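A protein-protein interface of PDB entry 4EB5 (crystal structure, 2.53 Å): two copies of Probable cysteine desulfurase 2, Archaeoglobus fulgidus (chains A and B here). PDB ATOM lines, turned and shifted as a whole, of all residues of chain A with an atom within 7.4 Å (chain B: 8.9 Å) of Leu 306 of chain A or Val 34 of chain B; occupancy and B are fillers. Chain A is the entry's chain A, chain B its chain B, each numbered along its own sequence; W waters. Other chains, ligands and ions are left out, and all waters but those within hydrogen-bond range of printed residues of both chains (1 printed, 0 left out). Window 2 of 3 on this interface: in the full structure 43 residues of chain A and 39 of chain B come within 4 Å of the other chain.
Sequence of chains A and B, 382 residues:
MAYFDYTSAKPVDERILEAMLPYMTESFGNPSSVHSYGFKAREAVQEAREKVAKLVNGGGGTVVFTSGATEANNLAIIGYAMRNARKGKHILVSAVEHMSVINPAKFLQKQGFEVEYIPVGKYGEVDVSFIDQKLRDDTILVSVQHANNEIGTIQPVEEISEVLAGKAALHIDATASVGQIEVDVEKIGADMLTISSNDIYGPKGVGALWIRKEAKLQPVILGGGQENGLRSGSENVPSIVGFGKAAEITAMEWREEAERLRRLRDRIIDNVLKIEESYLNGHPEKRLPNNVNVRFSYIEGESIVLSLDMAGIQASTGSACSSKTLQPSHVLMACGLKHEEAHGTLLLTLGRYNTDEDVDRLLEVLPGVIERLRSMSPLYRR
The side-chain carboxylate of Asp 5 of chain A sits at hydrogen-bond distance from a ring nitrogen (NE2) of His 35 of chain B (2.5 Å).
The side-chain carboxylate (OD2) of Asp 309 of chain A is in hydrogen-bond range of the backbone NH (N) of Ser 36 of chain B, 2.8 Å away.
The side-chain amide nitrogen of Gln 314 of chain A sits at hydrogen-bond distance from the side-chain carboxylate of Asp 309 of chain A (3.4 Å).
The side-chain hydroxyl of Ser 33 of chain B lies close to the backbone carbonyl oxygen of Asn 30 of chain B, 3.3 Å away.
ND1 of His 35 of chain B lies close to N of Tyr 37 of chain B (3.4 Å).
A ring nitrogen (ND1) of His 35 of chain B is in hydrogen-bond range of the backbone NH (N) of Gly 38 of chain B (3.4 Å).
OG of Ser 33 of chain B touches OD2 of Asp 5 of chain A (3.5 Å).
Val 305 of chain A touches Val 34 of chain B (CG1 to O, 3.5 Å).
CD1 of Leu 306 of chain A touches CG1 of Val 34 of chain B, 3.7 Å away.
Asp 309 of chain A touches His 35 of chain B (OD2 to CA, 3.4 Å).
Gln 314 of chain A touches His 35 of chain B.
Tyr 37 of chain B touches Gln 314 of chain A.
His 35 of chain B touches Ala 315 of chain A.
Val 305 of chain A touches one residue of chain B.
Leu 306 of chain A touches just one residue of chain B: Val 34.
No residue of chain B comes within 4 Å of Ser 307 of chain A.
Of the printed residues of chain B, Gln 314 of chain A touches His 35 (3.7 Å) and Tyr 37 (3.6 Å).
Of the printed residues of chain B, Ala 315 of chain A touches His 35.
Ser 316 of chain A touches none of the printed residues of chain B.
Of the printed residues of chain A, Ser 33 of chain B touches Asp 5.
Of chain A, only Val 305 and Leu 306 come within 4 Å of Val 34 of chain B.
Printed residues of chain A within 4 Å of His 35 of chain B: Asp 5, Asp 309, Gln 314 and Ala 315.
Printed residues of chain A within 4 Å of Tyr 37 of chain B: Gln 314.
The nearest residue of chain A that does not touch Val 34 of chain B is Glu 302 of chain A (4.1 Å).
The nearest printed residue of chain A that does not touch Ser 36 of chain B is Gln 314 of chain A (4.1 Å).
Printed residues of chain B that touch a printed residue of chain A: Ser 33, Val 34, His 35, Ser 36 and Tyr 37.
Along chain B the printed residues that touch a printed residue of chain A span positions 33 to 37.
Of the 24 printed residues of chain A, 6 touch a printed residue of chain B.
No position is printed for both chains.
Of the 9 pairs that touch across the chains among the printed residues, none has its exchanged pair printed and touching as well.
Water W1 lies within hydrogen-bond range of the backbone carbonyl oxygen (O) of Ala 315 of chain A (2.9 Å) and the backbone NH (N) of Val 34 of chain B (3.2 Å).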
ATOM      1  N   ASP A   5     -17.601 -16.780 -11.137  1.00  0.00           N
ATOM      2  CA  ASP A   5     -17.684 -16.941  -9.703  1.00  0.00           C
ATOM      3  C   ASP A   5     -19.135 -16.849  -9.137  1.00  0.00           C
ATOM      4  O   ASP A   5     -19.365 -16.662  -7.937  1.00  0.00           O
ATOM      5  CB  ASP A   5     -16.713 -15.960  -9.045  1.00  0.00           C
ATOM      6  CG  ASP A   5     -16.284 -16.387  -7.651  1.00  0.00           C
ATOM      7  OD1 ASP A   5     -16.620 -17.516  -7.182  1.00  0.00           O
ATOM      8  OD2 ASP A   5     -15.618 -15.569  -6.987  1.00  0.00           O
ATOM      9  N   GLU A 300      -0.484 -24.034  -6.412  1.00  0.00           N
ATOM     10  CA  GLU A 300      -1.375 -23.602  -5.364  1.00  0.00           C
ATOM     11  C   GLU A 300      -2.567 -22.758  -5.892  1.00  0.00           C
ATOM     12  O   GLU A 300      -2.398 -21.839  -6.721  1.00  0.00           O
ATOM     13  CB  GLU A 300      -0.555 -22.840  -4.333  1.00  0.00           C
ATOM     14  CG  GLU A 300      -1.265 -22.564  -3.031  1.00  0.00           C
ATOM     15  CD  GLU A 300      -2.214 -21.418  -3.135  1.00  0.00           C
ATOM     16  OE1 GLU A 300      -3.373 -21.532  -2.647  1.00  0.00           O
ATOM     17  OE2 GLU A 300      -1.804 -20.402  -3.743  1.00  0.00           O
ATOM     18  N   GLY A 301      -3.756 -23.065  -5.342  1.00  0.00           N
ATOM     19  CA  GLY A 301      -5.054 -22.451  -5.687  1.00  0.00           C
ATOM     20  C   GLY A 301      -5.251 -20.952  -5.673  1.00  0.00           C
ATOM     21  O   GLY A 301      -5.741 -20.383  -6.648  1.00  0.00           O
ATOM     22  N   GLU A 302      -4.910 -20.296  -4.579  1.00  0.00           N
ATOM     23  CA  GLU A 302      -4.954 -18.826  -4.561  1.00  0.00           C
ATOM     24  C   GLU A 302      -4.140 -18.185  -5.740  1.00  0.00           C
ATOM     25  O   GLU A 302      -4.578 -17.205  -6.323  1.00  0.00           O
ATOM     26  CB  GLU A 302      -4.544 -18.256  -3.181  1.00  0.00           C
ATOM     27  CG  GLU A 302      -4.631 -16.719  -3.112  1.00  0.00           C
ATOM     28  CD  GLU A 302      -3.818 -16.086  -1.987  1.00  0.00           C
ATOM     29  OE1 GLU A 302      -2.700 -15.535  -2.227  1.00  0.00           O
ATOM     30  OE2 GLU A 302      -4.304 -16.117  -0.852  1.00  0.00           O
ATOM     31  N   SER A 303      -2.991 -18.763  -6.088  1.00  0.00           N
ATOM     32  CA  SER A 303      -2.143 -18.269  -7.186  1.00  0.00           C
ATOM     33  C   SER A 303      -2.734 -18.471  -8.576  1.00  0.00           C
ATOM     34  O   SER A 303      -2.546 -17.614  -9.434  1.00  0.00           O
ATOM     35  CB  SER A 303      -0.757 -18.913  -7.142  1.00  0.00           C
ATOM     36  OG  SER A 303       0.026 -18.386  -6.092  1.00  0.00           O
ATOM     37  N   ILE A 304      -3.431 -19.587  -8.807  1.00  0.00           N
ATOM     38  CA  ILE A 304      -4.203 -19.751 -10.044  1.00  0.00           C
ATOM     39  C   ILE A 304      -5.289 -18.682 -10.110  1.00  0.00           C
ATOM     40  O   ILE A 304      -5.460 -18.031 -11.125  1.00  0.00           O
ATOM     41  CB  ILE A 304      -4.874 -21.123 -10.156  1.00  0.00           C
ATOM     42  CG1 ILE A 304      -3.856 -22.248 -10.143  1.00  0.00           C
ATOM     43  CG2 ILE A 304      -5.673 -21.224 -11.446  1.00  0.00           C
ATOM     44  CD1 ILE A 304      -4.398 -23.520  -9.471  1.00  0.00           C
ATOM     45  N   VAL A 305      -5.989 -18.468  -9.000  1.00  0.00           N
ATOM     46  CA  VAL A 305      -7.157 -17.573  -8.998  1.00  0.00           C
ATOM     47  C   VAL A 305      -6.777 -16.126  -9.245  1.00  0.00           C
ATOM     48  O   VAL A 305      -7.536 -15.388  -9.902  1.00  0.00           O
ATOM     49  CB  VAL A 305      -8.054 -17.785  -7.737  1.00  0.00           C
ATOM     50  CG1 VAL A 305      -8.892 -16.553  -7.374  1.00  0.00           C
ATOM     51  CG2 VAL A 305      -8.928 -18.981  -7.960  1.00  0.00           C
ATOM     52  N   LEU A 306      -5.607 -15.732  -8.743  1.00  0.00           N
ATOM     53  CA  LEU A 306      -5.144 -14.342  -8.899  1.00  0.00           C
ATOM     54  C   LEU A 306      -4.454 -14.070 -10.223  1.00  0.00           C
ATOM     55  O   LEU A 306      -4.393 -12.917 -10.655  1.00  0.00           O
ATOM     56  CB  LEU A 306      -4.259 -13.893  -7.727  1.00  0.00           C
ATOM     57  CG  LEU A 306      -5.053 -13.282  -6.590  1.00  0.00           C
ATOM     58  CD1 LEU A 306      -4.361 -13.495  -5.245  1.00  0.00           C
ATOM     59  CD2 LEU A 306      -5.190 -11.810  -6.915  1.00  0.00           C
ATOM     60  N   SER A 307      -3.914 -15.120 -10.848  1.00  0.00           N
ATOM     61  CA  SER A 307      -3.316 -14.990 -12.178  1.00  0.00           C
ATOM     62  C   SER A 307      -4.458 -14.734 -13.157  1.00  0.00           C
ATOM     63  O   SER A 307      -4.397 -13.814 -13.987  1.00  0.00           O
ATOM     64  CB  SER A 307      -2.559 -16.265 -12.593  1.00  0.00           C
ATOM     65  OG  SER A 307      -1.429 -16.556 -11.768  1.00  0.00           O
ATOM     66  N   LEU A 308      -5.512 -15.547 -13.031  1.00  0.00           N
ATOM     67  CA  LEU A 308      -6.726 -15.370 -13.818  1.00  0.00           C
ATOM     68  C   LEU A 308      -7.308 -13.960 -13.642  1.00  0.00           C
ATOM     69  O   LEU A 308      -7.785 -13.347 -14.619  1.00  0.00           O
ATOM     70  CB  LEU A 308      -7.761 -16.438 -13.455  1.00  0.00           C
ATOM     71  CG  LEU A 308      -7.543 -17.909 -13.852  1.00  0.00           C
ATOM     72  CD1 LEU A 308      -8.648 -18.812 -13.194  1.00  0.00           C
ATOM     73  CD2 LEU A 308      -7.481 -18.126 -15.399  1.00  0.00           C
ATOM     74  N   ASP A 309      -7.241 -13.438 -12.410  1.00  0.00           N
ATOM     75  CA  ASP A 309      -7.801 -12.127 -12.120  1.00  0.00           C
ATOM     76  C   ASP A 309      -7.014 -10.979 -12.752  1.00  0.00           C
ATOM     77  O   ASP A 309      -7.616  -9.986 -13.134  1.00  0.00           O
ATOM     78  CB  ASP A 309      -7.988 -11.894 -10.627  1.00  0.00           C
ATOM     79  CG  ASP A 309      -8.839 -10.662 -10.326  1.00  0.00           C
ATOM     80  OD1 ASP A 309      -9.848 -10.403 -11.026  1.00  0.00           O
ATOM     81  OD2 ASP A 309      -8.506  -9.937  -9.376  1.00  0.00           O
ATOM     82  N   MET A 310      -5.690 -11.107 -12.851  1.00  0.00           N
ATOM     83  CA  MET A 310      -4.888 -10.154 -13.672  1.00  0.00           C
ATOM     84  C   MET A 310      -5.205 -10.184 -15.163  1.00  0.00           C
ATOM     85  O   MET A 310      -5.115  -9.166 -15.802  1.00  0.00           O
ATOM     86  CB  MET A 310      -3.386 -10.280 -13.437  1.00  0.00           C
ATOM     87  CG  MET A 310      -2.857  -9.166 -12.501  1.00  0.00           C
ATOM     88  SD  MET A 310      -1.632  -9.659 -11.221  1.00  0.00           S
ATOM     89  CE  MET A 310      -1.202  -8.022 -10.577  1.00  0.00           C
ATOM     90  N   ALA A 311      -5.599 -11.341 -15.695  1.00  0.00           N
ATOM     91  CA  ALA A 311      -6.110 -11.459 -17.064  1.00  0.00           C
ATOM     92  C   ALA A 311      -7.559 -10.958 -17.230  1.00  0.00           C
ATOM     93  O   ALA A 311      -8.014 -10.716 -18.337  1.00  0.00           O
ATOM     94  CB  ALA A 311      -5.988 -12.901 -17.535  1.00  0.00           C
ATOM     95  N   GLY A 312      -8.285 -10.812 -16.123  1.00  0.00           N
ATOM     96  CA  GLY A 312      -9.692 -10.416 -16.185  1.00  0.00           C
ATOM     97  C   GLY A 312     -10.696 -11.549 -15.955  1.00  0.00           C
ATOM     98  O   GLY A 312     -11.798 -11.532 -16.487  1.00  0.00           O
ATOM     99  N   ILE A 313     -10.338 -12.523 -15.138  1.00  0.00           N
ATOM    100  CA  ILE A 313     -11.174 -13.685 -14.974  1.00  0.00           C
ATOM    101  C   ILE A 313     -11.350 -13.984 -13.495  1.00  0.00           C
ATOM    102  O   ILE A 313     -10.377 -14.274 -12.813  1.00  0.00           O
ATOM    103  CB  ILE A 313     -10.550 -14.905 -15.705  1.00  0.00           C
ATOM    104  CG1 ILE A 313     -10.618 -14.707 -17.229  1.00  0.00           C
ATOM    105  CG2 ILE A 313     -11.244 -16.173 -15.286  1.00  0.00           C
ATOM    106  CD1 ILE A 313      -9.754 -15.660 -18.057  1.00  0.00           C
ATOM    107  N   GLN A 314     -12.592 -13.937 -13.012  1.00  0.00           N
ATOM    108  CA  GLN A 314     -12.905 -14.192 -11.595  1.00  0.00           C
ATOM    109  C   GLN A 314     -13.253 -15.657 -11.342  1.00  0.00           C
ATOM    110  O   GLN A 314     -14.110 -16.230 -12.011  1.00  0.00           O
ATOM    111  CB  GLN A 314     -14.048 -13.309 -11.122  1.00  0.00           C
ATOM    112  CG  GLN A 314     -13.786 -11.819 -11.252  1.00  0.00           C
ATOM    113  CD  GLN A 314     -13.698 -11.351 -12.718  1.00  0.00           C
ATOM    114  OE1 GLN A 314     -14.624 -11.576 -13.520  1.00  0.00           O
ATOM    115  NE2 GLN A 314     -12.565 -10.715 -13.073  1.00  0.00           N
ATOM    116  N   ALA A 315     -12.557 -16.269 -10.385  1.00  0.00           N
ATOM    117  CA  ALA A 315     -12.805 -17.645 -10.012  1.00  0.00           C
ATOM    118  C   ALA A 315     -12.532 -17.853  -8.511  1.00  0.00           C
ATOM    119  O   ALA A 315     -12.464 -16.884  -7.731  1.00  0.00           O
ATOM    120  CB  ALA A 315     -11.978 -18.571 -10.874  1.00  0.00           C
ATOM    121  N   SER A 316     -12.331 -19.097  -8.110  1.00  0.00           N
ATOM    122  CA  SER A 316     -12.468 -19.506  -6.728  1.00  0.00           C
ATOM    123  C   SER A 316     -11.631 -20.775  -6.552  1.00  0.00           C
ATOM    124  O   SER A 316     -11.319 -21.466  -7.529  1.00  0.00           O
ATOM    125  CB  SER A 316     -13.954 -19.792  -6.462  1.00  0.00           C
ATOM    126  OG  SER A 316     -14.249 -19.873  -5.085  1.00  0.00           O
ATOM    127  N   THR A 317     -11.276 -21.061  -5.309  1.00  0.00           N
ATOM    128  CA  THR A 317     -10.404 -22.169  -4.964  1.00  0.00           C
ATOM    129  C   THR A 317     -10.813 -22.762  -3.597  1.00  0.00           C
ATOM    130  O   THR A 317     -11.478 -22.098  -2.788  1.00  0.00           O
ATOM    131  CB  THR A 317      -8.947 -21.694  -4.871  1.00  0.00           C
ATOM    132  OG1 THR A 317      -8.117 -22.756  -4.360  1.00  0.00           O
ATOM    133  CG2 THR A 317      -8.817 -20.468  -3.945  1.00  0.00           C
ATOM    134  N   CYS A 321      -4.546 -22.100   1.741  1.00  0.00           N
ATOM    135  CA  CYS A 321      -3.961 -20.761   1.479  1.00  0.00           C
ATOM    136  C   CYS A 321      -4.922 -19.584   1.223  1.00  0.00           C
ATOM    137  O   CYS A 321      -4.586 -18.435   1.466  1.00  0.00           O
ATOM    138  CB  CYS A 321      -2.961 -20.854   0.342  1.00  0.00           C
ATOM    139  SG  CYS A 321      -1.430 -21.706   0.819  1.00  0.00           S
ATOM    140  N   SER A 322      -6.123 -19.888   0.755  1.00  0.00           N
ATOM    141  CA  SER A 322      -7.154 -18.897   0.512  1.00  0.00           C
ATOM    142  C   SER A 322      -8.028 -18.569   1.748  1.00  0.00           C
ATOM    143  O   SER A 322      -8.749 -17.562   1.753  1.00  0.00           O
ATOM    144  CB  SER A 322      -8.055 -19.427  -0.615  1.00  0.00           C
ATOM    145  N   SER A 323      -8.010 -19.423   2.769  1.00  0.00           N
ATOM    146  CA  SER A 323      -9.064 -19.379   3.808  1.00  0.00           C
ATOM    147  C   SER A 323      -9.037 -18.164   4.736  1.00  0.00           C
ATOM    148  O   SER A 323     -10.039 -17.436   4.820  1.00  0.00           O
ATOM    149  CB  SER A 323      -9.128 -20.664   4.647  1.00  0.00           C
ATOM    150  N   VAL A 369      -1.241 -19.866 -17.593  1.00  0.00           N
ATOM    151  CA  VAL A 369      -1.193 -19.696 -16.148  1.00  0.00           C
ATOM    152  C   VAL A 369      -0.652 -20.960 -15.479  1.00  0.00           C
ATOM    153  O   VAL A 369       0.218 -20.898 -14.602  1.00  0.00           O
ATOM    154  CB  VAL A 369      -2.604 -19.400 -15.597  1.00  0.00           C
ATOM    155  CG1 VAL A 369      -2.672 -19.570 -14.036  1.00  0.00           C
ATOM    156  CG2 VAL A 369      -3.037 -18.017 -16.038  1.00  0.00           C
ATOM    157  N   LEU A 373       3.037 -20.967 -13.479  1.00  0.00           N
ATOM    158  CA  LEU A 373       3.142 -21.380 -12.098  1.00  0.00           C
ATOM    159  C   LEU A 373       3.915 -22.661 -11.980  1.00  0.00           C
ATOM    160  O   LEU A 373       4.741 -22.806 -11.088  1.00  0.00           O
ATOM    161  CB  LEU A 373       1.752 -21.527 -11.467  1.00  0.00           C
ATOM    162  CG  LEU A 373       0.984 -20.206 -11.367  1.00  0.00           C
ATOM    163  CD1 LEU A 373      -0.502 -20.481 -11.146  1.00  0.00           C
ATOM    164  CD2 LEU A 373       1.560 -19.378 -10.249  1.00  0.00           C
ATOM    165  N   ASN B  30     -18.581 -10.630  -3.799  1.00  0.00           N
ATOM    166  CA  ASN B  30     -18.584 -11.080  -2.425  1.00  0.00           C
ATOM    167  C   ASN B  30     -17.270 -10.704  -1.693  1.00  0.00           C
ATOM    168  O   ASN B  30     -16.177 -11.153  -2.059  1.00  0.00           O
ATOM    169  CB  ASN B  30     -18.753 -12.592  -2.439  1.00  0.00           C
ATOM    170  CG  ASN B  30     -18.882 -13.191  -1.055  1.00  0.00           C
ATOM    171  OD1 ASN B  30     -18.209 -12.781  -0.128  1.00  0.00           O
ATOM    172  ND2 ASN B  30     -19.732 -14.187  -0.920  1.00  0.00           N
ATOM    173  N   PRO B  31     -17.377  -9.903  -0.614  1.00  0.00           N
ATOM    174  CA  PRO B  31     -16.159  -9.471   0.076  1.00  0.00           C
ATOM    175  C   PRO B  31     -15.168 -10.600   0.441  1.00  0.00           C
ATOM    176  O   PRO B  31     -13.978 -10.323   0.576  1.00  0.00           O
ATOM    177  CB  PRO B  31     -16.683  -8.766   1.321  1.00  0.00           C
ATOM    178  CG  PRO B  31     -18.124  -9.006   1.357  1.00  0.00           C
ATOM    179  CD  PRO B  31     -18.591  -9.353   0.007  1.00  0.00           C
ATOM    180  N   SER B  32     -15.629 -11.842   0.592  1.00  0.00           N
ATOM    181  CA  SER B  32     -14.718 -12.967   0.882  1.00  0.00           C
ATOM    182  C   SER B  32     -13.865 -13.385  -0.331  1.00  0.00           C
ATOM    183  O   SER B  32     -12.862 -14.089  -0.181  1.00  0.00           O
ATOM    184  CB  SER B  32     -15.485 -14.192   1.362  1.00  0.00           C
ATOM    185  OG  SER B  32     -16.134 -13.915   2.584  1.00  0.00           O
ATOM    186  N   SER B  33     -14.264 -12.974  -1.529  1.00  0.00           N
ATOM    187  CA  SER B  33     -13.590 -13.438  -2.729  1.00  0.00           C
ATOM    188  C   SER B  33     -12.195 -12.847  -2.864  1.00  0.00           C
ATOM    189  O   SER B  33     -11.970 -11.694  -2.515  1.00  0.00           O
ATOM    190  CB  SER B  33     -14.420 -13.125  -3.958  1.00  0.00           C
ATOM    191  OG  SER B  33     -15.645 -13.839  -3.895  1.00  0.00           O
ATOM    192  N   VAL B  34     -11.267 -13.667  -3.348  1.00  0.00           N
ATOM    193  CA  VAL B  34      -9.916 -13.243  -3.642  1.00  0.00           C
ATOM    194  C   VAL B  34      -9.823 -12.818  -5.097  1.00  0.00           C
ATOM    195  O   VAL B  34      -9.134 -13.429  -5.876  1.00  0.00           O
ATOM    196  CB  VAL B  34      -8.897 -14.365  -3.368  1.00  0.00           C
ATOM    197  CG1 VAL B  34      -7.499 -13.778  -3.300  1.00  0.00           C
ATOM    198  CG2 VAL B  34      -9.231 -15.057  -2.047  1.00  0.00           C
ATOM    199  N   HIS B  35     -10.571 -11.805  -5.482  1.00  0.00           N
ATOM    200  CA  HIS B  35     -10.334 -11.181  -6.768  1.00  0.00           C
ATOM    201  C   HIS B  35     -10.808  -9.764  -6.657  1.00  0.00           C
ATOM    202  O   HIS B  35     -11.298  -9.365  -5.585  1.00  0.00           O
ATOM    203  CB  HIS B  35     -11.000 -11.929  -7.932  1.00  0.00           C
ATOM    204  CG  HIS B  35     -12.389 -12.414  -7.650  1.00  0.00           C
ATOM    205  ND1 HIS B  35     -13.468 -11.568  -7.539  1.00  0.00           N
ATOM    206  CD2 HIS B  35     -12.880 -13.668  -7.508  1.00  0.00           C
ATOM    207  CE1 HIS B  35     -14.556 -12.274  -7.302  1.00  0.00           C
ATOM    208  NE2 HIS B  35     -14.228 -13.550  -7.304  1.00  0.00           N
ATOM    209  N   SER B  36     -10.613  -9.010  -7.745  1.00  0.00           N
ATOM    210  CA  SER B  36     -11.086  -7.616  -7.887  1.00  0.00           C
ATOM    211  C   SER B  36     -12.553  -7.376  -7.496  1.00  0.00           C
ATOM    212  O   SER B  36     -12.848  -6.443  -6.748  1.00  0.00           O
ATOM    213  CB  SER B  36     -10.798  -7.088  -9.293  1.00  0.00           C
ATOM    214  OG  SER B  36     -11.286  -7.971 -10.291  1.00  0.00           O
ATOM    215  N   TYR B  37     -13.473  -8.230  -7.937  1.00  0.00           N
ATOM    216  CA  TYR B  37     -14.877  -8.065  -7.503  1.00  0.00           C
ATOM    217  C   TYR B  37     -15.023  -8.160  -5.989  1.00  0.00           C
ATOM    218  O   TYR B  37     -15.699  -7.347  -5.388  1.00  0.00           O
ATOM    219  CB  TYR B  37     -15.809  -9.055  -8.208  1.00  0.00           C
ATOM    220  CG  TYR B  37     -16.132  -8.691  -9.654  1.00  0.00           C
ATOM    221  CD1 TYR B  37     -15.121  -8.509 -10.594  1.00  0.00           C
ATOM    222  CD2 TYR B  37     -17.462  -8.559 -10.082  1.00  0.00           C
ATOM    223  CE1 TYR B  37     -15.413  -8.203 -11.929  1.00  0.00           C
ATOM    224  CE2 TYR B  37     -17.766  -8.247 -11.410  1.00  0.00           C
ATOM    225  CZ  TYR B  37     -16.741  -8.070 -12.327  1.00  0.00           C
ATOM    226  OH  TYR B  37     -17.050  -7.778 -13.639  1.00  0.00           O
ATOM    227  N   GLY B  38     -14.352  -9.129  -5.370  1.00  0.00           N
ATOM    228  CA  GLY B  38     -14.314  -9.207  -3.915  1.00  0.00           C
ATOM    229  C   GLY B  38     -13.621  -8.001  -3.270  1.00  0.00           C
ATOM    230  O   GLY B  38     -14.151  -7.408  -2.319  1.00  0.00           O
ATOM    231  N   PHE B  39     -12.449  -7.625  -3.805  1.00  0.00           N
ATOM    232  CA  PHE B  39     -11.684  -6.459  -3.324  1.00  0.00           C
ATOM    233  C   PHE B  39     -12.465  -5.169  -3.352  1.00  0.00           C
ATOM    234  O   PHE B  39     -12.452  -4.431  -2.397  1.00  0.00           O
ATOM    235  CB  PHE B  39     -10.379  -6.302  -4.087  1.00  0.00           C
ATOM    236  CG  PHE B  39      -9.506  -7.523  -4.046  1.00  0.00           C
ATOM    237  CD1 PHE B  39      -9.565  -8.419  -2.955  1.00  0.00           C
ATOM    238  CD2 PHE B  39      -8.613  -7.789  -5.101  1.00  0.00           C
ATOM    239  CE1 PHE B  39      -8.741  -9.562  -2.933  1.00  0.00           C
ATOM    240  CE2 PHE B  39      -7.794  -8.909  -5.096  1.00  0.00           C
ATOM    241  CZ  PHE B  39      -7.847  -9.798  -4.003  1.00  0.00           C
ATOM    242  N   LYS B  40     -13.180  -4.908  -4.433  1.00  0.00           N
ATOM    243  CA  LYS B  40     -14.048  -3.737  -4.477  1.00  0.00           C
ATOM    244  C   LYS B  40     -15.153  -3.823  -3.379  1.00  0.00           C
ATOM    245  O   LYS B  40     -15.442  -2.835  -2.686  1.00  0.00           O
ATOM    246  CB  LYS B  40     -14.627  -3.565  -5.899  1.00  0.00           C
ATOM    247  CG  LYS B  40     -15.404  -2.271  -6.167  1.00  0.00           C
ATOM    248  CD  LYS B  40     -14.621  -1.040  -5.745  1.00  0.00           C
ATOM    249  N   ARG B  42     -15.018  -5.433  -0.590  1.00  0.00           N
ATOM    250  CA  ARG B  42     -14.315  -5.192   0.672  1.00  0.00           C
ATOM    251  C   ARG B  42     -14.153  -3.701   1.056  1.00  0.00           C
ATOM    252  O   ARG B  42     -14.478  -3.298   2.175  1.00  0.00           O
ATOM    253  CB  ARG B  42     -12.952  -5.887   0.642  1.00  0.00           C
ATOM    254  CG  ARG B  42     -12.630  -6.691   1.896  1.00  0.00           C
HETATM  255  O   HOH W   1     -12.513 -16.087  -4.974  1.00  0.00           O
